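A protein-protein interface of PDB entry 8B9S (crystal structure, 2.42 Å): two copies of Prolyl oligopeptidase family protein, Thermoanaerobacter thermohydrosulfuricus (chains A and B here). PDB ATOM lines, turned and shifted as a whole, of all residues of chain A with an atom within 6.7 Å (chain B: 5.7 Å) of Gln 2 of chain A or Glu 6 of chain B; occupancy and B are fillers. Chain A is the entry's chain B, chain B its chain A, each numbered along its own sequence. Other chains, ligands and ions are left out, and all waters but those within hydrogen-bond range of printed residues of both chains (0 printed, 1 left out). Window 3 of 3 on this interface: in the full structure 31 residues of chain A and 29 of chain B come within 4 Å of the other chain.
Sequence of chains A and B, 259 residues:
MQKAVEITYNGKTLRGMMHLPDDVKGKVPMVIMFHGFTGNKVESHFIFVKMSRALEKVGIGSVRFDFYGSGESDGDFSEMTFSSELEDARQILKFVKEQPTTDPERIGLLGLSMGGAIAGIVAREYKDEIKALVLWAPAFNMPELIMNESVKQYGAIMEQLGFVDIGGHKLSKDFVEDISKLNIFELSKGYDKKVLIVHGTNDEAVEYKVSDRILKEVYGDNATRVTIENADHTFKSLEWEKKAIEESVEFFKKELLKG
Of the 14 printed residues of chain B, 6 touch a printed residue of chain A. Along chain B the printed residues that touch a printed residue of chain A span positions 4 to 74. Hydrophobic or aromatic side chains of chain A that line the printed part of chain B: Ala 4 and Met 17. Among the printed residues, 10 pairs touch across the chains. Among the printed residues, Asp or Glu carboxylates within 4 Å of a Lys or Arg side-chain nitrogen of the other chain: Arg 53 of chain A with Asp 74 of chain B (3.8 Å) and Arg 64 of chain A with Glu 72 of chain B (2.8 Å).
Ala 4 of chain B touches its own counterpart, Ala 4 of chain A. 1 position is printed for both chains.
NH1 of Arg 15 of chain B lies within hydrogen-bond range of OE1 of Gln 2 of chain A (3.4 Å). The guanidinium group (NH2) of Arg 53 of chain A lies within hydrogen-bond range of the backbone carbonyl oxygen (O) of Ser 73 of chain B. NH2 of Arg 64 of chain A is in salt-bridge range of OE1 of Glu 72 of chain B (2.8 Å). The side-chain carboxylate (OE1) of Glu 72 of chain B is in hydrogen-bond range of the side-chain amide nitrogen (NE2) of Gln 2 of chain A, at 2.8 Å. The backbone carbonyl oxygen (O) of Glu 72 of chain B sits at hydrogen-bond distance from the guanidinium group (NH2) of Arg 53 of chain A (3.2 Å). OD1 of Asp 74 of chain B is in salt-bridge range of NH2 of Arg 53 of chain A (3.8 Å).
The backbone NH (N) of Arg 15 of chain B sits at hydrogen-bond distance from the side-chain hydroxyl (OG) of Ser 73 of chain B. The guanidinium group (NH1) of Arg 15 of chain B is in salt-bridge range of the side-chain carboxylate (OD1) of Asp 74 of chain B (2.8 Å). The guanidinium group (NH2) of Arg 53 of chain A sits at hydrogen-bond distance from the side-chain amide oxygen (OE1) of Gln 2 of chain A (3.0 Å). The guanidinium group (NH1) of Arg 15 of chain B is in hydrogen-bond range of the backbone carbonyl oxygen (O) of Glu 72 of chain B (2.8 Å). The side-chain amide nitrogen of Gln 2 of chain A is in hydrogen-bond range of the side-chain sulfur of Met 17 of chain A (3.7 Å). NE of Arg 15 of chain B is in salt-bridge range of OE2 of Glu 6 of chain B (3.8 Å).
Gln 2 of chain A touches three residues of chain B. Of the printed residues of chain A, Ala 4 of chain B touches Ala 4 (3.4 Å). Glu 6 of chain B touches just one residue of chain A: Gln 2. Of the printed residues of chain A, Glu 72 of chain B touches Gln 2, Met 17, Arg 53 and Arg 64. Of the printed residues of chain A, Asp 74 of chain B touches Arg 53 (3.7 Å). The nearest residue of chain B that does not touch Gln 2 of chain A is Asp 74 of chain B (4.6 Å). The nearest printed residue of chain A that does not touch Ser 73 of chain B is Val 49 of chain A (5.2 Å).
Gln 2 of chain A touches Glu 6 of chain B. CB of Ala 4 of chain A touches CB of Ala 4 of chain B, 3.4 Å away. OE1 of Glu 72 of chain B touches CG of Met 17 of chain A, at 3.2 Å. NH1 of Arg 15 of chain B touches NH2 of Arg 53 of chain A, 3.5 Å away.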
ATOM      1  N   MET A   1      -5.154   7.614 -16.454  1.00  0.00           N
ATOM      2  CA  MET A   1      -3.942   7.393 -15.679  1.00  0.00           C
ATOM      3  C   MET A   1      -2.767   8.064 -16.379  1.00  0.00           C
ATOM      4  O   MET A   1      -2.712   8.118 -17.610  1.00  0.00           O
ATOM      5  CB  MET A   1      -3.658   5.901 -15.501  1.00  0.00           C
ATOM      6  CG  MET A   1      -3.167   5.216 -16.772  1.00  0.00           C
ATOM      7  SD  MET A   1      -1.362   5.204 -17.000  1.00  0.00           S
ATOM      8  CE  MET A   1      -0.953   3.855 -15.895  1.00  0.00           C
ATOM      9  N   GLN A   2      -1.854   8.613 -15.585  1.00  0.00           N
ATOM     10  CA  GLN A   2      -0.657   9.262 -16.100  1.00  0.00           C
ATOM     11  C   GLN A   2       0.548   8.712 -15.358  1.00  0.00           C
ATOM     12  O   GLN A   2       0.590   8.748 -14.126  1.00  0.00           O
ATOM     13  CB  GLN A   2      -0.757  10.775 -15.936  1.00  0.00           C
ATOM     14  CG  GLN A   2       0.457  11.532 -16.408  1.00  0.00           C
ATOM     15  CD  GLN A   2       0.228  13.031 -16.402  1.00  0.00           C
ATOM     16  OE1 GLN A   2      -0.894  13.502 -16.152  1.00  0.00           O
ATOM     17  NE2 GLN A   2       1.292  13.792 -16.640  1.00  0.00           N
ATOM     18  N   LYS A   3       1.518   8.194 -16.102  1.00  0.00           N
ATOM     19  CA  LYS A   3       2.721   7.660 -15.483  1.00  0.00           C
ATOM     20  C   LYS A   3       3.954   8.096 -16.269  1.00  0.00           C
ATOM     21  O   LYS A   3       3.935   8.150 -17.504  1.00  0.00           O
ATOM     22  CB  LYS A   3       2.680   6.125 -15.387  1.00  0.00           C
ATOM     23  CG  LYS A   3       2.788   5.410 -16.727  1.00  0.00           C
ATOM     24  CD  LYS A   3       2.944   3.892 -16.567  1.00  0.00           C
ATOM     25  CE  LYS A   3       3.189   3.228 -17.917  1.00  0.00           C
ATOM     26  NZ  LYS A   3       3.489   1.775 -17.766  1.00  0.00           N
ATOM     27  N   ALA A   4       5.028   8.383 -15.540  1.00  0.00           N
ATOM     28  CA  ALA A   4       6.315   8.682 -16.147  1.00  0.00           C
ATOM     29  C   ALA A   4       6.939   7.429 -16.762  1.00  0.00           C
ATOM     30  O   ALA A   4       6.910   6.348 -16.175  1.00  0.00           O
ATOM     31  CB  ALA A   4       7.248   9.256 -15.087  1.00  0.00           C
ATOM     32  N   MET A  17       5.985  10.851 -20.631  1.00  0.00           N
ATOM     33  CA  MET A  17       4.731  10.604 -19.935  1.00  0.00           C
ATOM     34  C   MET A  17       3.807   9.767 -20.805  1.00  0.00           C
ATOM     35  O   MET A  17       3.738   9.955 -22.026  1.00  0.00           O
ATOM     36  CB  MET A  17       4.023  11.926 -19.560  1.00  0.00           C
ATOM     37  CG  MET A  17       4.606  12.616 -18.364  1.00  0.00           C
ATOM     38  SD  MET A  17       4.259  11.608 -16.921  1.00  0.00           S
ATOM     39  CE  MET A  17       5.241  12.424 -15.665  1.00  0.00           C
ATOM     40  N   MET A  18       3.101   8.845 -20.163  1.00  0.00           N
ATOM     41  CA  MET A  18       2.148   7.958 -20.812  1.00  0.00           C
ATOM     42  C   MET A  18       0.789   8.117 -20.145  1.00  0.00           C
ATOM     43  O   MET A  18       0.685   8.072 -18.914  1.00  0.00           O
ATOM     44  CB  MET A  18       2.639   6.512 -20.739  1.00  0.00           C
ATOM     45  CG  MET A  18       1.758   5.480 -21.435  1.00  0.00           C
ATOM     46  SD  MET A  18       2.641   3.921 -21.470  1.00  0.00           S
ATOM     47  CE  MET A  18       1.377   2.788 -22.042  1.00  0.00           C
ATOM     48  N   HIS A  19      -0.234   8.327 -20.966  1.00  0.00           N
ATOM     49  CA  HIS A  19      -1.617   8.516 -20.555  1.00  0.00           C
ATOM     50  C   HIS A  19      -2.438   7.341 -21.068  1.00  0.00           C
ATOM     51  O   HIS A  19      -2.375   7.022 -22.265  1.00  0.00           O
ATOM     52  CB  HIS A  19      -2.182   9.815 -21.137  1.00  0.00           C
ATOM     53  CG  HIS A  19      -1.611  11.061 -20.533  1.00  0.00           C
ATOM     54  ND1 HIS A  19      -2.210  11.719 -19.479  1.00  0.00           N
ATOM     55  CD2 HIS A  19      -0.459  11.727 -20.787  1.00  0.00           C
ATOM     56  CE1 HIS A  19      -1.481  12.770 -19.148  1.00  0.00           C
ATOM     57  NE2 HIS A  19      -0.409  12.796 -19.921  1.00  0.00           N
ATOM     58  N   LEU A  20      -3.196   6.701 -20.171  1.00  0.00           N
ATOM     59  CA  LEU A  20      -4.139   5.661 -20.556  1.00  0.00           C
ATOM     60  C   LEU A  20      -5.521   5.983 -19.999  1.00  0.00           C
ATOM     61  O   LEU A  20      -5.638   6.499 -18.884  1.00  0.00           O
ATOM     62  CB  LEU A  20      -3.704   4.280 -20.052  1.00  0.00           C
ATOM     63  CG  LEU A  20      -2.417   3.657 -20.581  1.00  0.00           C
ATOM     64  CD1 LEU A  20      -2.108   2.343 -19.855  1.00  0.00           C
ATOM     65  CD2 LEU A  20      -2.501   3.451 -22.072  1.00  0.00           C
ATOM     66  N   ASP A  22      -8.805   5.513 -17.999  1.00  0.00           N
ATOM     67  CA  ASP A  22      -9.064   4.707 -16.808  1.00  0.00           C
ATOM     68  C   ASP A  22     -10.123   3.638 -17.055  1.00  0.00           C
ATOM     69  O   ASP A  22      -9.966   2.487 -16.621  1.00  0.00           O
ATOM     70  CB  ASP A  22      -9.540   5.612 -15.664  1.00  0.00           C
ATOM     71  CG  ASP A  22      -8.459   6.537 -15.156  1.00  0.00           C
ATOM     72  OD1 ASP A  22      -7.276   6.158 -15.221  1.00  0.00           O
ATOM     73  OD2 ASP A  22      -8.794   7.644 -14.683  1.00  0.00           O
ATOM     74  N   VAL A  49      -0.001  18.468 -22.709  1.00  0.00           N
ATOM     75  CA  VAL A  49      -0.597  17.825 -21.540  1.00  0.00           C
ATOM     76  C   VAL A  49      -2.114  17.835 -21.674  1.00  0.00           C
ATOM     77  O   VAL A  49      -2.779  16.796 -21.563  1.00  0.00           O
ATOM     78  CB  VAL A  49      -0.132  18.531 -20.245  1.00  0.00           C
ATOM     79  CG1 VAL A  49      -0.821  17.941 -18.997  1.00  0.00           C
ATOM     80  CG2 VAL A  49       1.375  18.476 -20.100  1.00  0.00           C
ATOM     81  N   ARG A  53      -4.892  14.749 -21.904  1.00  0.00           N
ATOM     82  CA  ARG A  53      -6.046  14.547 -21.036  1.00  0.00           C
ATOM     83  C   ARG A  53      -7.321  14.496 -21.855  1.00  0.00           C
ATOM     84  O   ARG A  53      -8.138  13.588 -21.671  1.00  0.00           O
ATOM     85  CB  ARG A  53      -6.087  15.627 -19.953  1.00  0.00           C
ATOM     86  CG  ARG A  53      -4.976  15.372 -18.950  1.00  0.00           C
ATOM     87  CD  ARG A  53      -4.733  16.441 -17.903  1.00  0.00           C
ATOM     88  NE  ARG A  53      -3.613  15.994 -17.076  1.00  0.00           N
ATOM     89  CZ  ARG A  53      -2.930  16.751 -16.232  1.00  0.00           C
ATOM     90  NH1 ARG A  53      -3.184  18.042 -16.092  1.00  0.00           N
ATOM     91  NH2 ARG A  53      -1.945  16.202 -15.526  1.00  0.00           N
ATOM     92  N   GLU A  56      -7.655  11.009 -23.153  1.00  0.00           N
ATOM     93  CA  GLU A  56      -8.041   9.941 -22.223  1.00  0.00           C
ATOM     94  C   GLU A  56      -9.549   9.811 -22.181  1.00  0.00           C
ATOM     95  O   GLU A  56     -10.094   8.701 -22.238  1.00  0.00           O
ATOM     96  CB  GLU A  56      -7.561  10.197 -20.790  1.00  0.00           C
ATOM     97  CG  GLU A  56      -6.102  10.466 -20.539  1.00  0.00           C
ATOM     98  CD  GLU A  56      -5.796  10.464 -19.038  1.00  0.00           C
ATOM     99  OE1 GLU A  56      -6.665   9.988 -18.276  1.00  0.00           O
ATOM    100  OE2 GLU A  56      -4.744  11.008 -18.613  1.00  0.00           O
ATOM    101  N   ARG A  64       4.188  11.163 -24.721  1.00  0.00           N
ATOM    102  CA  ARG A  64       4.870  12.407 -25.002  1.00  0.00           C
ATOM    103  C   ARG A  64       6.220  12.320 -24.340  1.00  0.00           C
ATOM    104  O   ARG A  64       6.274  12.215 -23.113  1.00  0.00           O
ATOM    105  CB  ARG A  64       4.109  13.596 -24.395  1.00  0.00           C
ATOM    106  CG  ARG A  64       2.684  13.792 -24.847  1.00  0.00           C
ATOM    107  CD  ARG A  64       2.051  14.883 -24.006  1.00  0.00           C
ATOM    108  NE  ARG A  64       1.782  14.462 -22.628  1.00  0.00           N
ATOM    109  CZ  ARG A  64       2.360  14.999 -21.564  1.00  0.00           C
ATOM    110  NH1 ARG A  64       3.351  15.868 -21.657  1.00  0.00           N
ATOM    111  NH2 ARG A  64       1.904  14.670 -20.355  1.00  0.00           N
ATOM    112  N   ALA B   4      11.802  10.074 -11.802  1.00  0.00           N
ATOM    113  CA  ALA B   4      10.512  10.735 -11.671  1.00  0.00           C
ATOM    114  C   ALA B   4       9.862  10.415 -10.324  1.00  0.00           C
ATOM    115  O   ALA B   4       9.986   9.306  -9.805  1.00  0.00           O
ATOM    116  CB  ALA B   4       9.614  10.297 -12.824  1.00  0.00           C
ATOM    117  N   VAL B   5       9.176  11.402  -9.745  1.00  0.00           N
ATOM    118  CA  VAL B   5       8.493  11.223  -8.461  1.00  0.00           C
ATOM    119  C   VAL B   5       7.088  11.826  -8.502  1.00  0.00           C
ATOM    120  O   VAL B   5       6.756  12.626  -9.381  1.00  0.00           O
ATOM    121  CB  VAL B   5       9.308  11.833  -7.290  1.00  0.00           C
ATOM    122  CG1 VAL B   5      10.554  10.994  -7.010  1.00  0.00           C
ATOM    123  CG2 VAL B   5       9.712  13.258  -7.618  1.00  0.00           C
ATOM    124  N   GLU B   6       6.259  11.418  -7.532  1.00  0.00           N
ATOM    125  CA  GLU B   6       4.894  11.911  -7.340  1.00  0.00           C
ATOM    126  C   GLU B   6       4.629  12.211  -5.870  1.00  0.00           C
ATOM    127  O   GLU B   6       5.211  11.585  -4.978  1.00  0.00           O
ATOM    128  CB  GLU B   6       3.804  10.905  -7.752  1.00  0.00           C
ATOM    129  CG  GLU B   6       3.578  10.713  -9.217  1.00  0.00           C
ATOM    130  CD  GLU B   6       2.456   9.735  -9.467  1.00  0.00           C
ATOM    131  OE1 GLU B   6       1.990   9.112  -8.484  1.00  0.00           O
ATOM    132  OE2 GLU B   6       2.033   9.604 -10.642  1.00  0.00           O
ATOM    133  N   ILE B   7       3.674  13.117  -5.637  1.00  0.00           N
ATOM    134  CA  ILE B   7       3.095  13.380  -4.323  1.00  0.00           C
ATOM    135  C   ILE B   7       1.580  13.412  -4.476  1.00  0.00           C
ATOM    136  O   ILE B   7       1.058  14.061  -5.384  1.00  0.00           O
ATOM    137  CB  ILE B   7       3.597  14.722  -3.731  1.00  0.00           C
ATOM    138  CG1 ILE B   7       5.085  14.661  -3.411  1.00  0.00           C
ATOM    139  CG2 ILE B   7       2.818  15.110  -2.484  1.00  0.00           C
ATOM    140  CD1 ILE B   7       5.688  16.021  -3.058  1.00  0.00           C
ATOM    141  N   THR B   8       0.855  12.773  -3.568  1.00  0.00           N
ATOM    142  CA  THR B   8      -0.600  12.879  -3.593  1.00  0.00           C
ATOM    143  C   THR B   8      -1.093  13.318  -2.225  1.00  0.00           C
ATOM    144  O   THR B   8      -0.809  12.662  -1.219  1.00  0.00           O
ATOM    145  CB  THR B   8      -1.260  11.566  -4.007  1.00  0.00           C
ATOM    146  OG1 THR B   8      -0.747  11.169  -5.282  1.00  0.00           O
ATOM    147  CG2 THR B   8      -2.783  11.756  -4.125  1.00  0.00           C
ATOM    148  N   THR B  13      -2.450  15.389  -7.250  1.00  0.00           N
ATOM    149  CA  THR B  13      -1.198  14.722  -7.588  1.00  0.00           C
ATOM    150  C   THR B  13      -0.237  15.739  -8.184  1.00  0.00           C
ATOM    151  O   THR B  13      -0.581  16.444  -9.141  1.00  0.00           O
ATOM    152  CB  THR B  13      -1.430  13.548  -8.544  1.00  0.00           C
ATOM    153  OG1 THR B  13      -2.350  12.627  -7.943  1.00  0.00           O
ATOM    154  CG2 THR B  13      -0.129  12.804  -8.832  1.00  0.00           C
ATOM    155  N   LEU B  14       0.941  15.848  -7.572  1.00  0.00           N
ATOM    156  CA  LEU B  14       2.059  16.638  -8.060  1.00  0.00           C
ATOM    157  C   LEU B  14       3.072  15.686  -8.686  1.00  0.00           C
ATOM    158  O   LEU B  14       3.336  14.606  -8.141  1.00  0.00           O
ATOM    159  CB  LEU B  14       2.718  17.409  -6.918  1.00  0.00           C
ATOM    160  CG  LEU B  14       1.741  18.241  -6.095  1.00  0.00           C
ATOM    161  CD1 LEU B  14       2.433  18.862  -4.893  1.00  0.00           C
ATOM    162  CD2 LEU B  14       1.032  19.278  -6.950  1.00  0.00           C
ATOM    163  N   ARG B  15       3.621  16.074  -9.836  1.00  0.00           N
ATOM    164  CA  ARG B  15       4.602  15.245 -10.530  1.00  0.00           C
ATOM    165  C   ARG B  15       5.908  16.009 -10.632  1.00  0.00           C
ATOM    166  O   ARG B  15       5.915  17.204 -10.946  1.00  0.00           O
ATOM    167  CB  ARG B  15       4.093  14.820 -11.915  1.00  0.00           C
ATOM    168  CG  ARG B  15       2.906  13.907 -11.776  1.00  0.00           C
ATOM    169  CD  ARG B  15       2.314  13.410 -13.071  1.00  0.00           C
ATOM    170  NE  ARG B  15       1.118  12.644 -12.733  1.00  0.00           N
ATOM    171  CZ  ARG B  15      -0.094  13.169 -12.642  1.00  0.00           C
ATOM    172  NH1 ARG B  15      -0.321  14.439 -12.939  1.00  0.00           N
ATOM    173  NH2 ARG B  15      -1.101  12.409 -12.218  1.00  0.00           N
ATOM    174  N   GLY B  16       7.014  15.323 -10.343  1.00  0.00           N
ATOM    175  CA  GLY B  16       8.298  15.994 -10.369  1.00  0.00           C
ATOM    176  C   GLY B  16       9.477  15.108 -10.701  1.00  0.00           C
ATOM    177  O   GLY B  16       9.322  13.967 -11.136  1.00  0.00           O
ATOM    178  N   PHE B  65       9.249  20.007  -8.714  1.00  0.00           N
ATOM    179  CA  PHE B  65       7.924  19.539  -9.020  1.00  0.00           C
ATOM    180  C   PHE B  65       7.128  20.625  -9.746  1.00  0.00           C
ATOM    181  O   PHE B  65       7.394  21.821  -9.577  1.00  0.00           O
ATOM    182  CB  PHE B  65       7.088  19.136  -7.794  1.00  0.00           C
ATOM    183  CG  PHE B  65       7.497  17.871  -7.058  1.00  0.00           C
ATOM    184  CD1 PHE B  65       8.709  17.726  -6.429  1.00  0.00           C
ATOM    185  CD2 PHE B  65       6.593  16.808  -7.022  1.00  0.00           C
ATOM    186  CE1 PHE B  65       9.016  16.561  -5.737  1.00  0.00           C
ATOM    187  CE2 PHE B  65       6.909  15.634  -6.351  1.00  0.00           C
ATOM    188  CZ  PHE B  65       8.119  15.517  -5.703  1.00  0.00           C
ATOM    189  N   GLU B  72       3.093  18.985 -15.773  1.00  0.00           N
ATOM    190  CA  GLU B  72       2.713  17.579 -15.670  1.00  0.00           C
ATOM    191  C   GLU B  72       1.778  17.289 -14.503  1.00  0.00           C
ATOM    192  O   GLU B  72       1.105  16.245 -14.503  1.00  0.00           O
ATOM    193  CB  GLU B  72       3.950  16.691 -15.526  1.00  0.00           C
ATOM    194  CG  GLU B  72       4.904  16.643 -16.733  1.00  0.00           C
ATOM    195  CD  GLU B  72       4.282  16.042 -17.990  1.00  0.00           C
ATOM    196  OE1 GLU B  72       3.189  15.420 -17.935  1.00  0.00           O
ATOM    197  OE2 GLU B  72       4.948  16.101 -19.033  1.00  0.00           O
ATOM    198  N   SER B  73       1.712  18.166 -13.511  1.00  0.00           N
ATOM    199  CA  SER B  73       0.838  17.894 -12.378  1.00  0.00           C
ATOM    200  C   SER B  73      -0.625  17.964 -12.807  1.00  0.00           C
ATOM    201  O   SER B  73      -0.967  18.491 -13.875  1.00  0.00           O
ATOM    202  CB  SER B  73       1.105  18.885 -11.242  1.00  0.00           C
ATOM    203  OG  SER B  73       2.419  18.720 -10.736  1.00  0.00           O
ATOM    204  N   ASP B  74      -1.491  17.399 -11.965  1.00  0.00           N
ATOM    205  CA  ASP B  74      -2.928  17.493 -12.181  1.00  0.00           C
ATOM    206  C   ASP B  74      -3.371  18.949 -12.069  1.00  0.00           C
ATOM    207  O   ASP B  74      -2.611  19.832 -11.655  1.00  0.00           O
ATOM    208  CB  ASP B  74      -3.726  16.691 -11.141  1.00  0.00           C
ATOM    209  CG  ASP B  74      -3.486  15.204 -11.211  1.00  0.00           C
ATOM    210  OD1 ASP B  74      -3.008  14.689 -12.245  1.00  0.00           O
ATOM    211  OD2 ASP B  74      -3.836  14.527 -10.220  1.00  0.00           O
ATOM    212  N   PHE B  95       7.860  15.856   1.486  1.00  0.00           N
ATOM    213  CA  PHE B  95       8.322  14.723   0.689  1.00  0.00           C
ATOM    214  C   PHE B  95       9.825  14.590   0.731  1.00  0.00           C
ATOM    215  O   PHE B  95      10.366  13.490   0.924  1.00  0.00           O
ATOM    216  CB  PHE B  95       7.792  14.886  -0.768  1.00  0.00           C
ATOM    217  CG  PHE B  95       8.211  13.809  -1.756  1.00  0.00           C
ATOM    218  CD1 PHE B  95       7.568  12.587  -1.796  1.00  0.00           C
ATOM    219  CD2 PHE B  95       9.193  14.066  -2.697  1.00  0.00           C
ATOM    220  CE1 PHE B  95       7.927  11.625  -2.724  1.00  0.00           C
ATOM    221  CE2 PHE B  95       9.561  13.098  -3.623  1.00  0.00           C
ATOM    222  CZ  PHE B  95       8.923  11.883  -3.635  1.00  0.00           C
